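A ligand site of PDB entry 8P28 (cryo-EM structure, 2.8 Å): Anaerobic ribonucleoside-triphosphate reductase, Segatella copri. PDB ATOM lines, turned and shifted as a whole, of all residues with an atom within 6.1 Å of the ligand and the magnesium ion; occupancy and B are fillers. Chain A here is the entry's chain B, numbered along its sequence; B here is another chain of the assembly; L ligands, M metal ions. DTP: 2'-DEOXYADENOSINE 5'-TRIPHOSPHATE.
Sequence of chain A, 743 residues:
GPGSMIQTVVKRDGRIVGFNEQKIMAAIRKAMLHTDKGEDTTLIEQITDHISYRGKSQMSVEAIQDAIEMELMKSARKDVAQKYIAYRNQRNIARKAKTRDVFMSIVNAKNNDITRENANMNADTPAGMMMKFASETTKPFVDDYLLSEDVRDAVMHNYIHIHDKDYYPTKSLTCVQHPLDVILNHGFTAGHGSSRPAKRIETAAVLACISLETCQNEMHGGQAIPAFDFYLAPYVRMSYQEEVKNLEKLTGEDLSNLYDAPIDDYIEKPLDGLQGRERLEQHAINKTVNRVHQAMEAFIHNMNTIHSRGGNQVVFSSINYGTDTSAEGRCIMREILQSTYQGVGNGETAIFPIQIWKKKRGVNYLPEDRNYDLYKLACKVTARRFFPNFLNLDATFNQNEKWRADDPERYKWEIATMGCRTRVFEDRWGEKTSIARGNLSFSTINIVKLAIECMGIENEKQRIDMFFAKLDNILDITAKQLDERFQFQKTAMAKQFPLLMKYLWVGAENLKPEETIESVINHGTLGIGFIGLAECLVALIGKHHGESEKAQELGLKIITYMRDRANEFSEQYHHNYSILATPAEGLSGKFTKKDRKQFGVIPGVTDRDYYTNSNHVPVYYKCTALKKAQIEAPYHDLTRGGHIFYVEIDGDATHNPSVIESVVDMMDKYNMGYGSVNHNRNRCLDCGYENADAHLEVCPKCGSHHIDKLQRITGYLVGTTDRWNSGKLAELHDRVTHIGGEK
The magnesium ion is bound by O2B of the ligand (1.8 Å), OE2 of Glu 297 of chain B (2.2 Å), O3B of the ligand (2.3 Å) and O3A of the ligand (2.6 Å). Slightly farther from the magnesium ion lies OE1 of Gln 294 of chain B (2.7 Å).
The backbone NH (N) of Ser 195 is in hydrogen-bond range of the backbone carbonyl oxygen (O) of Phe 188, 2.9 Å away. The guanidinium group (NH1) of Arg 200 is in hydrogen-bond range of the side-chain amide oxygen (OE1) of Gln 294 of chain B, at 3.2 Å. The side-chain carboxylate (OE2) of Glu 297 of chain B sits close to the side-chain amide oxygen (OE1) of Gln 294 of chain B. NH1 of Arg 196 is in hydrogen-bond range of O of Gly 345 of chain B. The side-chain hydroxyl of Thr 305 of chain B is in hydrogen-bond range of the backbone carbonyl oxygen of His 301 of chain B (3.0 Å). The guanidinium group (NH2) of Arg 200 is in salt-bridge range of the side-chain carboxylate (OE2) of Glu 242 (3.4 Å). OE1 of Glu 297 of chain B is in salt-bridge range of NH2 of Arg 196. ND1 of His 301 of chain B sits at hydrogen-bond distance from O of Glu 297 of chain B, 2.8 Å away.
OG1 of Thr 203 lies within hydrogen-bond range of O2A of the ligand, 2.7 Å away. NE of Arg 196 lies within salt-bridge range of O1B of the ligand (3.9 Å). A nitrogen (N3) of the ligand sits at hydrogen-bond distance from the side-chain hydroxyl (OG) of Ser 195. N of Lys 199 lies within hydrogen-bond range of O1A of the ligand (2.4 Å). The guanidinium group (NH1) of Arg 200 lies within salt-bridge range of an oxygen (O2A) of the ligand, 3.8 Å away.
The nearest printed residue that does not touch the magnesium ion is Arg 200 (4.2 Å).
O of Pro 197 lies close to O5' of the ligand. Residues that only touch the ligand: Ala 198 (3.0 Å), Val 206 (3.2 Å), Ala 298 of chain B (3.2 Å), His 301 of chain B (3.5 Å) and Asn 302 of chain B (3.6 Å). Hydrophobic or aromatic side chains that line the ligand: Val 206, Ala 298 of chain B and His 301 of chain B. Within 4 Å of the ligand: Ser 195, Arg 196, Pro 197, Ala 198, Lys 199, Arg 200, Thr 203, Val 206, Glu 297 of chain B, Ala 298 of chain B, His 301 of chain B and Asn 302 of chain B.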
ATOM      1  N   PHE A 188     -13.271 -13.826 -27.594  1.00  0.00           N
ATOM      2  CA  PHE A 188     -11.823 -13.726 -27.695  1.00  0.00           C
ATOM      3  C   PHE A 188     -11.166 -14.291 -26.445  1.00  0.00           C
ATOM      4  O   PHE A 188     -11.640 -14.071 -25.323  1.00  0.00           O
ATOM      5  CB  PHE A 188     -11.366 -12.284 -27.963  1.00  0.00           C
ATOM      6  CG  PHE A 188     -11.279 -11.403 -26.752  1.00  0.00           C
ATOM      7  CD1 PHE A 188     -10.200 -11.477 -25.899  1.00  0.00           C
ATOM      8  CD2 PHE A 188     -12.245 -10.460 -26.513  1.00  0.00           C
ATOM      9  CE1 PHE A 188     -10.110 -10.665 -24.806  1.00  0.00           C
ATOM     10  CE2 PHE A 188     -12.162  -9.634 -25.413  1.00  0.00           C
ATOM     11  CZ  PHE A 188     -11.090  -9.738 -24.564  1.00  0.00           C
ATOM     12  N   SER A 194     -10.918 -15.224 -21.107  1.00  0.00           N
ATOM     13  CA  SER A 194     -11.838 -15.500 -22.208  1.00  0.00           C
ATOM     14  C   SER A 194     -13.063 -14.607 -22.075  1.00  0.00           C
ATOM     15  O   SER A 194     -13.455 -14.240 -20.964  1.00  0.00           O
ATOM     16  CB  SER A 194     -12.253 -16.971 -22.220  1.00  0.00           C
ATOM     17  OG  SER A 194     -13.130 -17.232 -23.303  1.00  0.00           O
ATOM     18  N   SER A 195     -13.645 -14.245 -23.218  1.00  0.00           N
ATOM     19  CA  SER A 195     -14.843 -13.408 -23.226  1.00  0.00           C
ATOM     20  C   SER A 195     -15.770 -13.824 -24.348  1.00  0.00           C
ATOM     21  O   SER A 195     -15.332 -14.071 -25.484  1.00  0.00           O
ATOM     22  CB  SER A 195     -14.468 -11.933 -23.379  1.00  0.00           C
ATOM     23  OG  SER A 195     -13.687 -11.492 -22.286  1.00  0.00           O
ATOM     24  N   ARG A 196     -17.067 -13.869 -24.031  1.00  0.00           N
ATOM     25  CA  ARG A 196     -18.127 -14.226 -24.973  1.00  0.00           C
ATOM     26  C   ARG A 196     -18.509 -13.005 -25.810  1.00  0.00           C
ATOM     27  O   ARG A 196     -17.995 -11.895 -25.625  1.00  0.00           O
ATOM     28  CB  ARG A 196     -19.327 -14.759 -24.199  1.00  0.00           C
ATOM     29  CG  ARG A 196     -19.094 -16.043 -23.464  1.00  0.00           C
ATOM     30  CD  ARG A 196     -20.388 -16.524 -22.837  1.00  0.00           C
ATOM     31  NE  ARG A 196     -20.879 -15.582 -21.832  1.00  0.00           N
ATOM     32  CZ  ARG A 196     -20.822 -15.762 -20.522  1.00  0.00           C
ATOM     33  NH1 ARG A 196     -20.325 -16.865 -19.986  1.00  0.00           N
ATOM     34  NH2 ARG A 196     -21.278 -14.808 -19.715  1.00  0.00           N
ATOM     35  N   PRO A 197     -19.445 -13.160 -26.753  1.00  0.00           N
ATOM     36  CA  PRO A 197     -19.915 -12.002 -27.536  1.00  0.00           C
ATOM     37  C   PRO A 197     -20.687 -10.986 -26.717  1.00  0.00           C
ATOM     38  O   PRO A 197     -20.834 -11.141 -25.498  1.00  0.00           O
ATOM     39  CB  PRO A 197     -20.820 -12.639 -28.599  1.00  0.00           C
ATOM     40  CG  PRO A 197     -20.346 -14.042 -28.704  1.00  0.00           C
ATOM     41  CD  PRO A 197     -19.916 -14.427 -27.333  1.00  0.00           C
ATOM     42  N   ALA A 198     -21.167  -9.933 -27.365  1.00  0.00           N
ATOM     43  CA  ALA A 198     -21.907  -8.865 -26.709  1.00  0.00           C
ATOM     44  C   ALA A 198     -23.406  -8.977 -27.006  1.00  0.00           C
ATOM     45  O   ALA A 198     -23.821  -9.553 -28.012  1.00  0.00           O
ATOM     46  CB  ALA A 198     -21.403  -7.495 -27.166  1.00  0.00           C
ATOM     47  N   LYS A 199     -24.215  -8.416 -26.097  1.00  0.00           N
ATOM     48  CA  LYS A 199     -25.665  -8.413 -26.295  1.00  0.00           C
ATOM     49  C   LYS A 199     -26.344  -7.114 -25.864  1.00  0.00           C
ATOM     50  O   LYS A 199     -27.545  -7.109 -25.607  1.00  0.00           O
ATOM     51  CB  LYS A 199     -26.300  -9.587 -25.546  1.00  0.00           C
ATOM     52  CG  LYS A 199     -26.142 -10.913 -26.246  1.00  0.00           C
ATOM     53  CD  LYS A 199     -27.093 -11.928 -25.660  1.00  0.00           C
ATOM     54  CE  LYS A 199     -26.958 -13.269 -26.358  1.00  0.00           C
ATOM     55  NZ  LYS A 199     -27.887 -14.280 -25.782  1.00  0.00           N
ATOM     56  N   ARG A 200     -25.609  -6.004 -25.788  1.00  0.00           N
ATOM     57  CA  ARG A 200     -26.202  -4.714 -25.456  1.00  0.00           C
ATOM     58  C   ARG A 200     -25.094  -3.674 -25.523  1.00  0.00           C
ATOM     59  O   ARG A 200     -23.927  -3.992 -25.762  1.00  0.00           O
ATOM     60  CB  ARG A 200     -26.870  -4.721 -24.083  1.00  0.00           C
ATOM     61  CG  ARG A 200     -25.963  -5.147 -22.951  1.00  0.00           C
ATOM     62  CD  ARG A 200     -26.787  -5.400 -21.711  1.00  0.00           C
ATOM     63  NE  ARG A 200     -27.589  -6.605 -21.859  1.00  0.00           N
ATOM     64  CZ  ARG A 200     -27.300  -7.779 -21.331  1.00  0.00           C
ATOM     65  NH1 ARG A 200     -26.249  -7.958 -20.558  1.00  0.00           N
ATOM     66  NH2 ARG A 200     -28.100  -8.810 -21.589  1.00  0.00           N
ATOM     67  N   THR A 203     -21.991  -3.574 -22.731  1.00  0.00           N
ATOM     68  CA  THR A 203     -20.988  -4.612 -22.886  1.00  0.00           C
ATOM     69  C   THR A 203     -20.304  -4.572 -24.236  1.00  0.00           C
ATOM     70  O   THR A 203     -19.676  -5.557 -24.624  1.00  0.00           O
ATOM     71  CB  THR A 203     -21.622  -5.987 -22.677  1.00  0.00           C
ATOM     72  OG1 THR A 203     -20.591  -6.981 -22.648  1.00  0.00           O
ATOM     73  CG2 THR A 203     -22.590  -6.300 -23.801  1.00  0.00           C
ATOM     74  N   VAL A 206     -17.159  -1.401 -23.508  1.00  0.00           N
ATOM     75  CA  VAL A 206     -16.191  -1.987 -22.576  1.00  0.00           C
ATOM     76  C   VAL A 206     -15.244  -2.920 -23.319  1.00  0.00           C
ATOM     77  O   VAL A 206     -14.028  -2.873 -23.126  1.00  0.00           O
ATOM     78  CB  VAL A 206     -16.921  -2.711 -21.436  1.00  0.00           C
ATOM     79  CG1 VAL A 206     -15.937  -3.426 -20.547  1.00  0.00           C
ATOM     80  CG2 VAL A 206     -17.731  -1.730 -20.620  1.00  0.00           C
ATOM     81  N   LEU A 207     -15.786  -3.773 -24.185  1.00  0.00           N
ATOM     82  CA  LEU A 207     -14.922  -4.671 -24.947  1.00  0.00           C
ATOM     83  C   LEU A 207     -14.047  -3.893 -25.933  1.00  0.00           C
ATOM     84  O   LEU A 207     -12.893  -4.268 -26.160  1.00  0.00           O
ATOM     85  CB  LEU A 207     -15.744  -5.708 -25.695  1.00  0.00           C
ATOM     86  CG  LEU A 207     -16.553  -6.696 -24.837  1.00  0.00           C
ATOM     87  CD1 LEU A 207     -17.051  -7.830 -25.702  1.00  0.00           C
ATOM     88  CD2 LEU A 207     -15.739  -7.222 -23.685  1.00  0.00           C
ATOM     89  N   ILE A 210     -11.234  -2.684 -23.870  1.00  0.00           N
ATOM     90  CA  ILE A 210     -10.361  -3.804 -23.518  1.00  0.00           C
ATOM     91  C   ILE A 210      -9.423  -4.112 -24.675  1.00  0.00           C
ATOM     92  O   ILE A 210      -8.204  -4.244 -24.483  1.00  0.00           O
ATOM     93  CB  ILE A 210     -11.200  -5.032 -23.130  1.00  0.00           C
ATOM     94  CG1 ILE A 210     -11.918  -4.797 -21.800  1.00  0.00           C
ATOM     95  CG2 ILE A 210     -10.333  -6.266 -23.071  1.00  0.00           C
ATOM     96  CD1 ILE A 210     -11.005  -4.731 -20.612  1.00  0.00           C
ATOM     97  N   GLU A 242     -34.851  -5.368 -25.880  1.00  0.00           N
ATOM     98  CA  GLU A 242     -34.950  -5.833 -24.500  1.00  0.00           C
ATOM     99  C   GLU A 242     -35.860  -4.943 -23.676  1.00  0.00           C
ATOM    100  O   GLU A 242     -36.645  -5.431 -22.854  1.00  0.00           O
ATOM    101  CB  GLU A 242     -33.564  -5.915 -23.856  1.00  0.00           C
ATOM    102  CG  GLU A 242     -32.785  -7.163 -24.246  1.00  0.00           C
ATOM    103  CD  GLU A 242     -31.575  -7.384 -23.359  1.00  0.00           C
ATOM    104  OE1 GLU A 242     -31.373  -6.616 -22.408  1.00  0.00           O
ATOM    105  OE2 GLU A 242     -30.817  -8.351 -23.627  1.00  0.00           O
ATOM    106  N   HIS B 293     -26.457  -8.721 -11.016  1.00  0.00           N
ATOM    107  CA  HIS B 293     -25.880  -9.918 -11.614  1.00  0.00           C
ATOM    108  C   HIS B 293     -24.860  -9.558 -12.691  1.00  0.00           C
ATOM    109  O   HIS B 293     -23.714 -10.047 -12.678  1.00  0.00           O
ATOM    110  CB  HIS B 293     -27.004 -10.778 -12.181  1.00  0.00           C
ATOM    111  CG  HIS B 293     -26.556 -12.094 -12.735  1.00  0.00           C
ATOM    112  ND1 HIS B 293     -25.846 -12.219 -13.905  1.00  0.00           N
ATOM    113  CD2 HIS B 293     -26.762 -13.354 -12.288  1.00  0.00           C
ATOM    114  CE1 HIS B 293     -25.623 -13.494 -14.154  1.00  0.00           C
ATOM    115  NE2 HIS B 293     -26.165 -14.202 -13.189  1.00  0.00           N
ATOM    116  N   GLN B 294     -25.260  -8.698 -13.623  1.00  0.00           N
ATOM    117  CA  GLN B 294     -24.368  -8.312 -14.707  1.00  0.00           C
ATOM    118  C   GLN B 294     -23.129  -7.601 -14.177  1.00  0.00           C
ATOM    119  O   GLN B 294     -22.016  -7.850 -14.637  1.00  0.00           O
ATOM    120  CB  GLN B 294     -25.106  -7.423 -15.702  1.00  0.00           C
ATOM    121  CG  GLN B 294     -26.400  -8.012 -16.259  1.00  0.00           C
ATOM    122  CD  GLN B 294     -26.180  -9.270 -17.065  1.00  0.00           C
ATOM    123  OE1 GLN B 294     -25.268  -9.353 -17.882  1.00  0.00           O
ATOM    124  NE2 GLN B 294     -27.032 -10.261 -16.851  1.00  0.00           N
ATOM    125  N   GLU B 297     -20.706 -10.163 -12.584  1.00  0.00           N
ATOM    126  CA  GLU B 297     -19.986 -10.979 -13.551  1.00  0.00           C
ATOM    127  C   GLU B 297     -18.998 -10.147 -14.362  1.00  0.00           C
ATOM    128  O   GLU B 297     -17.905 -10.645 -14.686  1.00  0.00           O
ATOM    129  CB  GLU B 297     -20.952 -11.721 -14.479  1.00  0.00           C
ATOM    130  CG  GLU B 297     -21.478 -10.952 -15.669  1.00  0.00           C
ATOM    131  CD  GLU B 297     -22.221 -11.864 -16.628  1.00  0.00           C
ATOM    132  OE1 GLU B 297     -22.283 -13.076 -16.343  1.00  0.00           O
ATOM    133  OE2 GLU B 297     -22.740 -11.365 -17.657  1.00  0.00           O
ATOM    134  N   ALA B 298     -19.325  -8.895 -14.662  1.00  0.00           N
ATOM    135  CA  ALA B 298     -18.378  -8.027 -15.349  1.00  0.00           C
ATOM    136  C   ALA B 298     -17.145  -7.748 -14.500  1.00  0.00           C
ATOM    137  O   ALA B 298     -16.025  -7.728 -15.019  1.00  0.00           O
ATOM    138  CB  ALA B 298     -19.056  -6.717 -15.739  1.00  0.00           C
ATOM    139  N   PHE B 299     -17.324  -7.532 -13.199  1.00  0.00           N
ATOM    140  CA  PHE B 299     -16.189  -7.367 -12.295  1.00  0.00           C
ATOM    141  C   PHE B 299     -15.299  -8.610 -12.306  1.00  0.00           C
ATOM    142  O   PHE B 299     -14.075  -8.529 -12.478  1.00  0.00           O
ATOM    143  CB  PHE B 299     -16.706  -7.077 -10.893  1.00  0.00           C
ATOM    144  CG  PHE B 299     -15.638  -7.039  -9.829  1.00  0.00           C
ATOM    145  CD1 PHE B 299     -15.252  -8.198  -9.180  1.00  0.00           C
ATOM    146  CD2 PHE B 299     -15.068  -5.845  -9.437  1.00  0.00           C
ATOM    147  CE1 PHE B 299     -14.290  -8.156  -8.202  1.00  0.00           C
ATOM    148  CE2 PHE B 299     -14.109  -5.813  -8.456  1.00  0.00           C
ATOM    149  CZ  PHE B 299     -13.732  -6.975  -7.837  1.00  0.00           C
ATOM    150  N   HIS B 301     -14.971 -10.917 -14.569  1.00  0.00           N
ATOM    151  CA  HIS B 301     -14.259 -11.064 -15.836  1.00  0.00           C
ATOM    152  C   HIS B 301     -13.148 -10.030 -15.974  1.00  0.00           C
ATOM    153  O   HIS B 301     -12.042 -10.359 -16.427  1.00  0.00           O
ATOM    154  CB  HIS B 301     -15.237 -10.945 -17.004  1.00  0.00           C
ATOM    155  CG  HIS B 301     -16.069 -12.171 -17.230  1.00  0.00           C
ATOM    156  ND1 HIS B 301     -16.805 -12.767 -16.231  1.00  0.00           N
ATOM    157  CD2 HIS B 301     -16.296 -12.905 -18.343  1.00  0.00           C
ATOM    158  CE1 HIS B 301     -17.450 -13.809 -16.719  1.00  0.00           C
ATOM    159  NE2 HIS B 301     -17.148 -13.911 -18.003  1.00  0.00           N
ATOM    160  N   ASN B 302     -13.415  -8.783 -15.606  1.00  0.00           N
ATOM    161  CA  ASN B 302     -12.437  -7.719 -15.793  1.00  0.00           C
ATOM    162  C   ASN B 302     -11.180  -7.974 -14.970  1.00  0.00           C
ATOM    163  O   ASN B 302     -10.068  -7.732 -15.435  1.00  0.00           O
ATOM    164  CB  ASN B 302     -13.050  -6.367 -15.433  1.00  0.00           C
ATOM    165  CG  ASN B 302     -12.074  -5.230 -15.524  1.00  0.00           C
ATOM    166  OD1 ASN B 302     -10.964  -5.300 -15.009  1.00  0.00           O
ATOM    167  ND2 ASN B 302     -12.477  -4.154 -16.186  1.00  0.00           N
ATOM    168  N   THR B 305      -8.903 -10.743 -16.712  1.00  0.00           N
ATOM    169  CA  THR B 305      -8.298 -10.475 -18.010  1.00  0.00           C
ATOM    170  C   THR B 305      -7.076  -9.577 -17.891  1.00  0.00           C
ATOM    171  O   THR B 305      -6.586  -9.088 -18.911  1.00  0.00           O
ATOM    172  CB  THR B 305      -9.330  -9.856 -18.951  1.00  0.00           C
ATOM    173  OG1 THR B 305     -10.516 -10.654 -18.959  1.00  0.00           O
ATOM    174  CG2 THR B 305      -8.787  -9.779 -20.372  1.00  0.00           C
ATOM    175  N   GLY B 345     -16.335 -17.322 -19.362  1.00  0.00           N
ATOM    176  CA  GLY B 345     -16.266 -17.790 -20.732  1.00  0.00           C
ATOM    177  C   GLY B 345     -17.250 -18.913 -20.973  1.00  0.00           C
ATOM    178  O   GLY B 345     -18.397 -18.839 -20.536  1.00  0.00           O
HETATM  179  PG  DTP L   1     -26.500 -13.431 -20.673  1.00  0.00           P
HETATM  180  O1G DTP L   1     -27.851 -13.026 -21.142  1.00  0.00           O
HETATM  181  O2G DTP L   1     -25.992 -14.692 -21.351  1.00  0.00           O
HETATM  182  O3G DTP L   1     -26.409 -13.585 -19.164  1.00  0.00           O
HETATM  183  PB  DTP L   1     -23.946 -12.210 -21.535  1.00  0.00           P
HETATM  184  O1B DTP L   1     -23.699 -13.050 -22.709  1.00  0.00           O
HETATM  185  O2B DTP L   1     -23.040 -12.474 -20.336  1.00  0.00           O
HETATM  186  O3B DTP L   1     -25.433 -12.329 -21.031  1.00  0.00           O
HETATM  187  PA  DTP L   1     -22.893  -9.728 -22.687  1.00  0.00           P
HETATM  188  O1A DTP L   1     -23.416  -9.488 -24.048  1.00  0.00           O
HETATM  189  O2A DTP L   1     -22.694  -8.462 -21.855  1.00  0.00           O
HETATM  190  O3A DTP L   1     -23.851 -10.658 -21.863  1.00  0.00           O
HETATM  191  O5' DTP L   1     -21.536 -10.541 -22.702  1.00  0.00           O
HETATM  192  C5' DTP L   1     -20.281  -9.883 -22.447  1.00  0.00           C
HETATM  193  C4' DTP L   1     -19.238 -10.932 -22.129  1.00  0.00           C
HETATM  194  O4' DTP L   1     -18.088 -10.219 -21.632  1.00  0.00           O
HETATM  195  C3' DTP L   1     -19.699 -11.781 -20.957  1.00  0.00           C
HETATM  196  O3' DTP L   1     -18.804 -12.893 -20.935  1.00  0.00           O
HETATM  197  C2' DTP L   1     -19.286 -10.917 -19.778  1.00  0.00           C
HETATM  198  C1' DTP L   1     -17.931 -10.435 -20.241  1.00  0.00           C
HETATM  199  N9  DTP L   1     -17.550  -9.157 -19.655  1.00  0.00           N
HETATM  200  C8  DTP L   1     -18.346  -8.257 -19.005  1.00  0.00           C
HETATM  201  N7  DTP L   1     -17.701  -7.188 -18.584  1.00  0.00           N
HETATM  202  C5  DTP L   1     -16.403  -7.412 -18.985  1.00  0.00           C
HETATM  203  C6  DTP L   1     -15.223  -6.657 -18.845  1.00  0.00           C
HETATM  204  N6  DTP L   1     -15.160  -5.472 -18.233  1.00  0.00           N
HETATM  205  N1  DTP L   1     -14.089  -7.166 -19.370  1.00  0.00           N
HETATM  206  C2  DTP L   1     -14.131  -8.346 -19.983  1.00  0.00           C
HETATM  207  N3  DTP L   1     -15.185  -9.149 -20.172  1.00  0.00           N
HETATM  208  C4  DTP L   1     -16.293  -8.616 -19.651  1.00  0.00           C
HETATM  209 MG    MG M   1     -24.119 -11.319 -19.378  1.00  0.00          MG
